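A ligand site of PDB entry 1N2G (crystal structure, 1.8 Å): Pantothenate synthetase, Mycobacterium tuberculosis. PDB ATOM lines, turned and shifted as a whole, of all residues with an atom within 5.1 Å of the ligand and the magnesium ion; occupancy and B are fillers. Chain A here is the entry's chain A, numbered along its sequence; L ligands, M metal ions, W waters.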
ATOM      1  N   PRO A  38     -20.034 -14.300 -21.132  1.00  0.00           N
ATOM      2  CA  PRO A  38     -21.362 -14.836 -20.840  1.00  0.00           C
ATOM      3  C   PRO A  38     -22.312 -13.730 -20.434  1.00  0.00           C
ATOM      4  O   PRO A  38     -21.994 -12.953 -19.526  1.00  0.00           O
ATOM      5  CB  PRO A  38     -21.111 -15.787 -19.666  1.00  0.00           C
ATOM      6  CG  PRO A  38     -19.638 -16.094 -19.768  1.00  0.00           C
ATOM      7  CD  PRO A  38     -19.067 -14.753 -20.125  1.00  0.00           C
ATOM      8  N   THR A  39     -23.469 -13.658 -21.088  1.00  0.00           N
ATOM      9  CA  THR A  39     -24.463 -12.637 -20.743  1.00  0.00           C
ATOM     10  C   THR A  39     -25.869 -13.244 -20.821  1.00  0.00           C
ATOM     11  O   THR A  39     -26.047 -14.369 -21.299  1.00  0.00           O
ATOM     12  CB  THR A  39     -24.448 -11.446 -21.728  1.00  0.00           C
ATOM     13  OG1 THR A  39     -25.232 -11.778 -22.891  1.00  0.00           O
ATOM     14  CG2 THR A  39     -23.016 -11.134 -22.159  1.00  0.00           C
ATOM     15  N   MET A  40     -26.844 -12.506 -20.302  1.00  0.00           N
ATOM     16  CA  MET A  40     -28.236 -12.939 -20.381  1.00  0.00           C
ATOM     17  C   MET A  40     -28.972 -11.948 -21.288  1.00  0.00           C
ATOM     18  O   MET A  40     -30.171 -11.719 -21.160  1.00  0.00           O
ATOM     19  CB  MET A  40     -28.866 -12.970 -18.991  1.00  0.00           C
ATOM     20  CG  MET A  40     -28.169 -13.972 -18.066  1.00  0.00           C
ATOM     21  SD  MET A  40     -29.279 -14.912 -16.967  1.00  0.00           S
ATOM     22  CE  MET A  40     -29.829 -13.591 -15.897  1.00  0.00           C
ATOM     23  N   GLY A  41     -28.224 -11.362 -22.226  1.00  0.00           N
ATOM     24  CA  GLY A  41     -28.821 -10.401 -23.148  1.00  0.00           C
ATOM     25  C   GLY A  41     -29.189  -9.047 -22.570  1.00  0.00           C
ATOM     26  O   GLY A  41     -28.780  -8.719 -21.450  1.00  0.00           O
ATOM     27  N   HIS A  44     -26.028  -3.546 -22.475  1.00  0.00           N
ATOM     28  CA  HIS A  44     -25.829  -2.124 -22.282  1.00  0.00           C
ATOM     29  C   HIS A  44     -24.323  -1.844 -22.196  1.00  0.00           C
ATOM     30  O   HIS A  44     -23.502  -2.764 -22.355  1.00  0.00           O
ATOM     31  CB  HIS A  44     -26.564  -1.640 -21.016  1.00  0.00           C
ATOM     32  CG  HIS A  44     -26.215  -2.407 -19.791  1.00  0.00           C
ATOM     33  ND1 HIS A  44     -24.952  -2.393 -19.228  1.00  0.00           N
ATOM     34  CD2 HIS A  44     -26.972  -3.204 -18.984  1.00  0.00           C
ATOM     35  CE1 HIS A  44     -24.944  -3.131 -18.137  1.00  0.00           C
ATOM     36  NE2 HIS A  44     -26.161  -3.632 -17.967  1.00  0.00           N
ATOM     37  N   GLY A  46     -22.305  -1.549 -19.901  1.00  0.00           N
ATOM     38  CA  GLY A  46     -21.571  -2.394 -18.971  1.00  0.00           C
ATOM     39  C   GLY A  46     -21.117  -3.671 -19.691  1.00  0.00           C
ATOM     40  O   GLY A  46     -19.960  -4.102 -19.563  1.00  0.00           O
ATOM     41  N   HIS A  47     -22.018  -4.275 -20.460  1.00  0.00           N
ATOM     42  CA  HIS A  47     -21.659  -5.487 -21.202  1.00  0.00           C
ATOM     43  C   HIS A  47     -20.590  -5.156 -22.243  1.00  0.00           C
ATOM     44  O   HIS A  47     -19.681  -5.945 -22.481  1.00  0.00           O
ATOM     45  CB  HIS A  47     -22.863  -6.073 -21.965  1.00  0.00           C
ATOM     46  CG  HIS A  47     -23.994  -6.499 -21.085  1.00  0.00           C
ATOM     47  ND1 HIS A  47     -25.028  -5.652 -20.760  1.00  0.00           N
ATOM     48  CD2 HIS A  47     -24.254  -7.676 -20.480  1.00  0.00           C
ATOM     49  CE1 HIS A  47     -25.891  -6.295 -19.988  1.00  0.00           C
ATOM     50  NE2 HIS A  47     -25.442  -7.528 -19.804  1.00  0.00           N
ATOM     51  N   LEU A  50     -17.053  -5.417 -21.160  1.00  0.00           N
ATOM     52  CA  LEU A  50     -16.565  -6.797 -21.149  1.00  0.00           C
ATOM     53  C   LEU A  50     -16.149  -7.193 -22.555  1.00  0.00           C
ATOM     54  O   LEU A  50     -15.083  -7.781 -22.769  1.00  0.00           O
ATOM     55  CB  LEU A  50     -17.659  -7.751 -20.655  1.00  0.00           C
ATOM     56  CG  LEU A  50     -17.719  -7.926 -19.126  1.00  0.00           C
ATOM     57  CD1 LEU A  50     -17.974  -6.608 -18.468  1.00  0.00           C
ATOM     58  CD2 LEU A  50     -18.826  -8.935 -18.749  1.00  0.00           C
ATOM     59  N   TYR A  82     -37.605 -10.967 -16.809  1.00  0.00           N
ATOM     60  CA  TYR A  82     -36.289 -10.568 -17.302  1.00  0.00           C
ATOM     61  C   TYR A  82     -36.373  -9.895 -18.667  1.00  0.00           C
ATOM     62  O   TYR A  82     -36.973 -10.433 -19.593  1.00  0.00           O
ATOM     63  CB  TYR A  82     -35.307 -11.736 -17.403  1.00  0.00           C
ATOM     64  CG  TYR A  82     -33.881 -11.231 -17.391  1.00  0.00           C
ATOM     65  CD1 TYR A  82     -33.307 -10.762 -16.211  1.00  0.00           C
ATOM     66  CD2 TYR A  82     -33.135 -11.129 -18.563  1.00  0.00           C
ATOM     67  CE1 TYR A  82     -32.015 -10.204 -16.204  1.00  0.00           C
ATOM     68  CE2 TYR A  82     -31.848 -10.569 -18.564  1.00  0.00           C
ATOM     69  CZ  TYR A  82     -31.310 -10.110 -17.380  1.00  0.00           C
ATOM     70  OH  TYR A  82     -30.055  -9.551 -17.375  1.00  0.00           O
ATOM     71  N   PRO A  83     -35.739  -8.729 -18.818  1.00  0.00           N
ATOM     72  CA  PRO A  83     -35.777  -8.019 -20.102  1.00  0.00           C
ATOM     73  C   PRO A  83     -35.132  -8.775 -21.261  1.00  0.00           C
ATOM     74  O   PRO A  83     -34.067  -9.391 -21.117  1.00  0.00           O
ATOM     75  CB  PRO A  83     -35.081  -6.694 -19.787  1.00  0.00           C
ATOM     76  CG  PRO A  83     -34.058  -7.104 -18.763  1.00  0.00           C
ATOM     77  CD  PRO A  83     -34.821  -8.059 -17.871  1.00  0.00           C
ATOM     78  N   PHE A 156     -14.814 -13.557 -19.264  1.00  0.00           N
ATOM     79  CA  PHE A 156     -14.969 -12.227 -18.681  1.00  0.00           C
ATOM     80  C   PHE A 156     -16.249 -12.014 -17.886  1.00  0.00           C
ATOM     81  O   PHE A 156     -17.349 -12.356 -18.358  1.00  0.00           O
ATOM     82  CB  PHE A 156     -14.890 -11.183 -19.819  1.00  0.00           C
ATOM     83  CG  PHE A 156     -13.581 -11.190 -20.565  1.00  0.00           C
ATOM     84  CD1 PHE A 156     -13.273 -12.229 -21.450  1.00  0.00           C
ATOM     85  CD2 PHE A 156     -12.612 -10.219 -20.299  1.00  0.00           C
ATOM     86  CE1 PHE A 156     -12.014 -12.303 -22.059  1.00  0.00           C
ATOM     87  CE2 PHE A 156     -11.350 -10.283 -20.907  1.00  0.00           C
ATOM     88  CZ  PHE A 156     -11.053 -11.330 -21.788  1.00  0.00           C
ATOM     89  N   PHE A 157     -16.091 -11.449 -16.696  1.00  0.00           N
ATOM     90  CA  PHE A 157     -17.208 -11.142 -15.808  1.00  0.00           C
ATOM     91  C   PHE A 157     -17.038  -9.738 -15.191  1.00  0.00           C
ATOM     92  O   PHE A 157     -15.921  -9.312 -14.916  1.00  0.00           O
ATOM     93  CB  PHE A 157     -17.278 -12.197 -14.690  1.00  0.00           C
ATOM     94  CG  PHE A 157     -17.837 -13.522 -15.151  1.00  0.00           C
ATOM     95  CD1 PHE A 157     -17.004 -14.551 -15.541  1.00  0.00           C
ATOM     96  CD2 PHE A 157     -19.222 -13.716 -15.208  1.00  0.00           C
ATOM     97  CE1 PHE A 157     -17.542 -15.779 -15.983  1.00  0.00           C
ATOM     98  CE2 PHE A 157     -19.758 -14.923 -15.656  1.00  0.00           C
ATOM     99  CZ  PHE A 157     -18.912 -15.957 -16.042  1.00  0.00           C
ATOM    100  N   GLY A 158     -18.141  -9.047 -14.960  1.00  0.00           N
ATOM    101  CA  GLY A 158     -18.049  -7.720 -14.383  1.00  0.00           C
ATOM    102  C   GLY A 158     -17.854  -7.707 -12.877  1.00  0.00           C
ATOM    103  O   GLY A 158     -18.342  -8.587 -12.149  1.00  0.00           O
ATOM    104  N   GLU A 159     -17.124  -6.714 -12.389  1.00  0.00           N
ATOM    105  CA  GLU A 159     -16.912  -6.591 -10.952  1.00  0.00           C
ATOM    106  C   GLU A 159     -18.218  -6.196 -10.264  1.00  0.00           C
ATOM    107  O   GLU A 159     -18.379  -6.389  -9.064  1.00  0.00           O
ATOM    108  CB  GLU A 159     -15.831  -5.560 -10.682  1.00  0.00           C
ATOM    109  CG  GLU A 159     -14.460  -6.178 -10.528  1.00  0.00           C
ATOM    110  CD  GLU A 159     -13.369  -5.144 -10.380  1.00  0.00           C
ATOM    111  OE1 GLU A 159     -13.659  -4.061  -9.847  1.00  0.00           O
ATOM    112  OE2 GLU A 159     -12.224  -5.430 -10.804  1.00  0.00           O
ATOM    113  N   LYS A 160     -19.155  -5.638 -11.030  1.00  0.00           N
ATOM    114  CA  LYS A 160     -20.441  -5.224 -10.453  1.00  0.00           C
ATOM    115  C   LYS A 160     -21.090  -6.351  -9.643  1.00  0.00           C
ATOM    116  O   LYS A 160     -21.611  -6.131  -8.553  1.00  0.00           O
ATOM    117  CB  LYS A 160     -21.406  -4.768 -11.554  1.00  0.00           C
ATOM    118  CG  LYS A 160     -22.690  -4.174 -10.981  1.00  0.00           C
ATOM    119  CD  LYS A 160     -23.709  -3.875 -12.055  1.00  0.00           C
ATOM    120  CE  LYS A 160     -24.435  -5.142 -12.477  1.00  0.00           C
ATOM    121  NZ  LYS A 160     -25.410  -4.865 -13.570  1.00  0.00           N
ATOM    122  N   ASP A 161     -21.082  -7.554 -10.200  1.00  0.00           N
ATOM    123  CA  ASP A 161     -21.639  -8.721  -9.536  1.00  0.00           C
ATOM    124  C   ASP A 161     -20.416  -9.427  -8.951  1.00  0.00           C
ATOM    125  O   ASP A 161     -20.018 -10.504  -9.388  1.00  0.00           O
ATOM    126  CB  ASP A 161     -22.356  -9.588 -10.572  1.00  0.00           C
ATOM    127  CG  ASP A 161     -23.553  -8.866 -11.178  1.00  0.00           C
ATOM    128  OD1 ASP A 161     -24.573  -8.742 -10.472  1.00  0.00           O
ATOM    129  OD2 ASP A 161     -23.462  -8.403 -12.338  1.00  0.00           O
ATOM    130  N   GLN A 164     -20.640 -13.015  -7.592  1.00  0.00           N
ATOM    131  CA  GLN A 164     -20.701 -13.949  -8.703  1.00  0.00           C
ATOM    132  C   GLN A 164     -19.293 -14.182  -9.266  1.00  0.00           C
ATOM    133  O   GLN A 164     -18.924 -15.307  -9.596  1.00  0.00           O
ATOM    134  CB  GLN A 164     -21.616 -13.393  -9.800  1.00  0.00           C
ATOM    135  CG  GLN A 164     -21.403 -14.030 -11.157  1.00  0.00           C
ATOM    136  CD  GLN A 164     -22.484 -13.640 -12.133  1.00  0.00           C
ATOM    137  OE1 GLN A 164     -23.587 -14.187 -12.111  1.00  0.00           O
ATOM    138  NE2 GLN A 164     -22.184 -12.662 -12.987  1.00  0.00           N
ATOM    139  N   VAL A 184     -13.782  -7.462 -14.841  1.00  0.00           N
ATOM    140  CA  VAL A 184     -13.790  -6.163 -15.496  1.00  0.00           C
ATOM    141  C   VAL A 184     -14.437  -5.082 -14.613  1.00  0.00           C
ATOM    142  O   VAL A 184     -15.527  -5.283 -14.076  1.00  0.00           O
ATOM    143  CB  VAL A 184     -14.550  -6.266 -16.838  1.00  0.00           C
ATOM    144  CG1 VAL A 184     -14.613  -4.891 -17.534  1.00  0.00           C
ATOM    145  CG2 VAL A 184     -13.858  -7.275 -17.735  1.00  0.00           C
ATOM    146  N   PRO A 185     -13.774  -3.916 -14.449  1.00  0.00           N
ATOM    147  CA  PRO A 185     -14.301  -2.822 -13.627  1.00  0.00           C
ATOM    148  C   PRO A 185     -15.725  -2.404 -13.968  1.00  0.00           C
ATOM    149  O   PRO A 185     -16.106  -2.375 -15.133  1.00  0.00           O
ATOM    150  CB  PRO A 185     -13.289  -1.697 -13.869  1.00  0.00           C
ATOM    151  CG  PRO A 185     -11.997  -2.472 -14.076  1.00  0.00           C
ATOM    152  CD  PRO A 185     -12.473  -3.542 -15.036  1.00  0.00           C
ATOM    153  N   THR A 186     -16.485  -2.058 -12.944  1.00  0.00           N
ATOM    154  CA  THR A 186     -17.866  -1.654 -13.134  1.00  0.00           C
ATOM    155  C   THR A 186     -18.041  -0.366 -13.938  1.00  0.00           C
ATOM    156  O   THR A 186     -17.351   0.634 -13.710  1.00  0.00           O
ATOM    157  CB  THR A 186     -18.555  -1.515 -11.765  1.00  0.00           C
ATOM    158  OG1 THR A 186     -18.620  -2.808 -11.151  1.00  0.00           O
ATOM    159  CG2 THR A 186     -19.953  -0.935 -11.891  1.00  0.00           C
ATOM    160  N   VAL A 187     -18.931  -0.414 -14.930  1.00  0.00           N
ATOM    161  CA  VAL A 187     -19.226   0.755 -15.752  1.00  0.00           C
ATOM    162  C   VAL A 187     -20.336   1.521 -15.056  1.00  0.00           C
ATOM    163  O   VAL A 187     -21.330   0.936 -14.632  1.00  0.00           O
ATOM    164  CB  VAL A 187     -19.691   0.351 -17.185  1.00  0.00           C
ATOM    165  CG1 VAL A 187     -20.019   1.592 -17.989  1.00  0.00           C
ATOM    166  CG2 VAL A 187     -18.598  -0.441 -17.879  1.00  0.00           C
ATOM    167  N   ALA A 194     -24.210   2.366 -10.908  1.00  0.00           N
ATOM    168  CA  ALA A 194     -23.694   1.210 -11.647  1.00  0.00           C
ATOM    169  C   ALA A 194     -24.704   0.829 -12.713  1.00  0.00           C
ATOM    170  O   ALA A 194     -25.884   0.646 -12.405  1.00  0.00           O
ATOM    171  CB  ALA A 194     -23.458   0.043 -10.710  1.00  0.00           C
ATOM    172  N   MET A 195     -24.265   0.708 -13.951  1.00  0.00           N
ATOM    173  CA  MET A 195     -25.205   0.324 -14.998  1.00  0.00           C
ATOM    174  C   MET A 195     -25.715  -1.092 -14.768  1.00  0.00           C
ATOM    175  O   MET A 195     -24.978  -1.993 -14.355  1.00  0.00           O
ATOM    176  CB  MET A 195     -24.570   0.447 -16.374  1.00  0.00           C
ATOM    177  CG  MET A 195     -24.603   1.882 -16.890  1.00  0.00           C
ATOM    178  SD  MET A 195     -23.742   2.035 -18.452  1.00  0.00           S
ATOM    179  CE  MET A 195     -23.475   3.812 -18.529  1.00  0.00           C
ATOM    180  N   SER A 196     -26.990  -1.281 -15.037  1.00  0.00           N
ATOM    181  CA  SER A 196     -27.625  -2.564 -14.804  1.00  0.00           C
ATOM    182  C   SER A 196     -28.919  -2.567 -15.595  1.00  0.00           C
ATOM    183  O   SER A 196     -29.580  -1.533 -15.701  1.00  0.00           O
ATOM    184  CB  SER A 196     -27.923  -2.692 -13.307  1.00  0.00           C
ATOM    185  OG  SER A 196     -28.341  -4.005 -12.966  1.00  0.00           O
ATOM    186  N   SER A 197     -29.297  -3.715 -16.136  1.00  0.00           N
ATOM    187  CA  SER A 197     -30.534  -3.773 -16.893  1.00  0.00           C
ATOM    188  C   SER A 197     -31.725  -3.496 -15.997  1.00  0.00           C
ATOM    189  O   SER A 197     -32.750  -3.004 -16.475  1.00  0.00           O
ATOM    190  CB  SER A 197     -30.680  -5.120 -17.588  1.00  0.00           C
ATOM    191  OG  SER A 197     -29.919  -5.116 -18.776  1.00  0.00           O
ATOM    192  N   ARG A 198     -31.588  -3.784 -14.707  1.00  0.00           N
ATOM    193  CA  ARG A 198     -32.698  -3.525 -13.790  1.00  0.00           C
ATOM    194  C   ARG A 198     -32.937  -2.016 -13.543  1.00  0.00           C
ATOM    195  O   ARG A 198     -33.968  -1.636 -12.986  1.00  0.00           O
ATOM    196  CB  ARG A 198     -32.443  -4.215 -12.454  1.00  0.00           C
ATOM    197  CG  ARG A 198     -31.320  -3.577 -11.666  1.00  0.00           C
ATOM    198  CD  ARG A 198     -30.947  -4.441 -10.484  1.00  0.00           C
ATOM    199  NE  ARG A 198     -30.348  -5.708 -10.913  1.00  0.00           N
ATOM    200  CZ  ARG A 198     -29.858  -6.622 -10.084  1.00  0.00           C
ATOM    201  NH1 ARG A 198     -29.899  -6.413  -8.777  1.00  0.00           N
ATOM    202  NH2 ARG A 198     -29.314  -7.728 -10.563  1.00  0.00           N
ATOM    203  N   ASN A 199     -31.987  -1.176 -13.957  1.00  0.00           N
ATOM    204  CA  ASN A 199     -32.120   0.265 -13.765  1.00  0.00           C
ATOM    205  C   ASN A 199     -33.322   0.799 -14.523  1.00  0.00           C
ATOM    206  O   ASN A 199     -33.860   1.860 -14.191  1.00  0.00           O
ATOM    207  CB  ASN A 199     -30.868   1.012 -14.257  1.00  0.00           C
ATOM    208  CG  ASN A 199     -29.688   0.839 -13.315  1.00  0.00           C
ATOM    209  OD1 ASN A 199     -29.826   0.245 -12.242  1.00  0.00           O
ATOM    210  ND2 ASN A 199     -28.529   1.368 -13.705  1.00  0.00           N
HETATM  211  P1  LIG L   1     -29.544  -7.067 -14.455  1.00  0.00           P
HETATM  212  O1  LIG L   1     -29.221  -8.180 -13.418  1.00  0.00           O
HETATM  213  O2  LIG L   1     -30.703  -7.515 -15.389  1.00  0.00           O
HETATM  214  O3  LIG L   1     -29.951  -5.758 -13.692  1.00  0.00           O
HETATM  215  P2  LIG L   1     -26.925  -7.501 -15.890  1.00  0.00           P
HETATM  216  O4  LIG L   1     -26.395  -6.792 -17.144  1.00  0.00           O
HETATM  217  O5  LIG L   1     -25.842  -7.464 -14.794  1.00  0.00           O
HETATM  218  O6  LIG L   1     -28.243  -6.727 -15.396  1.00  0.00           O
HETATM  219  P3  LIG L   1     -26.183  -9.963 -16.854  1.00  0.00           P
HETATM  220  O7  LIG L   1     -26.503 -10.243 -18.292  1.00  0.00           O
HETATM  221  O8  LIG L   1     -26.129 -11.131 -15.959  1.00  0.00           O
HETATM  222  C1  LIG L   1     -27.269  -8.980 -16.257  1.00  0.00           C
HETATM  223  O9  LIG L   1     -24.690  -9.440 -16.897  1.00  0.00           O
HETATM  224  C2  LIG L   1     -23.715 -10.138 -17.699  1.00  0.00           C
HETATM  225  C3  LIG L   1     -22.286  -9.716 -17.325  1.00  0.00           C
HETATM  226  O10 LIG L   1     -22.105  -8.291 -17.489  1.00  0.00           O
HETATM  227  C4  LIG L   1     -21.965 -10.030 -15.883  1.00  0.00           C
HETATM  228  O11 LIG L   1     -20.666 -10.615 -15.799  1.00  0.00           O
HETATM  229  C5  LIG L   1     -22.040  -8.695 -15.212  1.00  0.00           C
HETATM  230  O12 LIG L   1     -21.277  -8.616 -14.010  1.00  0.00           O
HETATM  231  C6  LIG L   1     -21.567  -7.760 -16.293  1.00  0.00           C
HETATM  232  N1  LIG L   1     -22.042  -6.404 -16.023  1.00  0.00           N
HETATM  233  C7  LIG L   1     -23.315  -5.911 -15.878  1.00  0.00           C
HETATM  234  N2  LIG L   1     -23.445  -4.647 -15.637  1.00  0.00           N
HETATM  235  C8  LIG L   1     -22.127  -4.226 -15.615  1.00  0.00           C
HETATM  236  C9  LIG L   1     -21.525  -2.962 -15.410  1.00  0.00           C
HETATM  237  N3  LIG L   1     -22.240  -1.854 -15.168  1.00  0.00           N
HETATM  238  N4  LIG L   1     -20.112  -2.886 -15.478  1.00  0.00           N
HETATM  239  C10 LIG L   1     -19.351  -3.997 -15.723  1.00  0.00           C
HETATM  240  N5  LIG L   1     -19.846  -5.262 -15.928  1.00  0.00           N
HETATM  241  C11 LIG L   1     -21.252  -5.298 -15.864  1.00  0.00           C
HETATM  242 MG    MG M   1     -27.292  -8.495 -13.419  1.00  0.00          MG
HETATM  243  O   HOH W   1     -19.656 -10.889 -12.334  1.00  0.00           O
HETATM  244  O   HOH W   2     -25.840  -9.773 -13.339  1.00  0.00           O
HETATM  245  O   HOH W   3     -26.697  -7.885 -11.638  1.00  0.00           O
HETATM  246  O   HOH W   4     -20.085 -12.105 -17.992  1.00  0.00           O
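A ring nitrogen (NE2) of His 47 lies within hydrogen-bond range of an oxygen (O4) of the ligand (2.9 Å).
An oxygen (O11) of the ligand is in hydrogen-bond range of the backbone NH (N) of Gly 158, at 3.1 Å.
A nitrogen (N4) of the ligand lies within hydrogen-bond range of the backbone NH (N) of Val 187.
The backbone carbonyl oxygen (O) of Gly 158 lies close to an oxygen (O12) of the ligand, 3.5 Å away.
The backbone NH (N) of Ser 197 sits at hydrogen-bond distance from an oxygen (O3) of the ligand.
The side-chain hydroxyl (OG) of Ser 196 sits at hydrogen-bond distance from an oxygen (O3) of the ligand.
A nitrogen (N2) of the ligand lies within hydrogen-bond range of the side-chain amino group (NZ) of Lys 160.
An oxygen (O4) of the ligand sits at hydrogen-bond distance from a ring nitrogen (NE2) of His 44 (3.3 Å).
The backbone carbonyl oxygen of Val 187 lies within hydrogen-bond range of a nitrogen (N3) of the ligand, 3.0 Å away.
N3 of the ligand is in hydrogen-bond range of O of Met 195.
The side-chain hydroxyl of Tyr 82 is in hydrogen-bond range of an oxygen (O2) of the ligand (2.9 Å).
OD2 of Asp 161 sits at hydrogen-bond distance from O12 of the ligand, 2.8 Å away.
An oxygen (O3) of the ligand is in hydrogen-bond range of the backbone NH of Arg 198 (2.8 Å).
N of Met 40 is in hydrogen-bond range of O7 of the ligand (3.0 Å).
O3 of the ligand lies within salt-bridge range of NE of Arg 198.
N of Ser 196 lies close to ND2 of Asn 199, at 3.3 Å.
The backbone carbonyl oxygen (O) of Val 187 sits at hydrogen-bond distance from the backbone NH (N) of Met 195 (3.0 Å).
The guanidinium group of Arg 198 lies close to the side-chain hydroxyl of Ser 196, 3.3 Å away.
The backbone NH (N) of Gly 41 lies within hydrogen-bond range of the side-chain hydroxyl (OG1) of Thr 39.
The backbone carbonyl oxygen of Phe 157 lies within hydrogen-bond range of the backbone NH of Val 184 (2.8 Å).
N of His 44 lies within hydrogen-bond range of ND1 of His 47 (2.9 Å).
The backbone carbonyl oxygen (O) of Met 195 sits at hydrogen-bond distance from the side-chain amino group (NZ) of Lys 160 (3.0 Å).
The side-chain hydroxyl (OG1) of Thr 186 is in hydrogen-bond range of the backbone NH (N) of Lys 160.
Residues that only touch the ligand: Pro 38 (3.8 Å), Thr 39 (3.98 Å), Gly 46 (3.6 Å), Leu 50 (3.4 Å), Phe 157 (3.5 Å), Gln 164 (3.8 Å), Pro 185 (3.7 Å) and Thr 186 (3.5 Å).
Merely in contact with the magnesium ion: Arg 198 (3.6 Å) and Asp 161 (3.98 Å).
The nearest printed residue that does not touch the magnesium ion is Lys 160 (4.1 Å).
The magnesium ion is bound by water W2, O1 of the ligand, water W3 and O5 of the ligand.
Slightly farther from the magnesium ion lies an oxygen (O6) of the ligand (2.8 Å).
Water W3 lies within hydrogen-bond range of the side-chain carboxylate of Asp 161 (2.6 Å) and the guanidinium group of Arg 198 (2.8 Å).
Water W2 bridges OD2 of Asp 161 (2.9 Å) and O8 of the ligand (3.0 Å).
Water W4 lies within hydrogen-bond range of the backbone carbonyl oxygen of Pro 38 (2.6 Å), an oxygen (O11) of the ligand (2.7 Å) and the backbone carbonyl oxygen of Phe 156 (2.8 Å).
Water W1 lies within hydrogen-bond range of O of Gly 158, O of Asp 161, NE2 of Gln 164 and O12 of the ligand.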
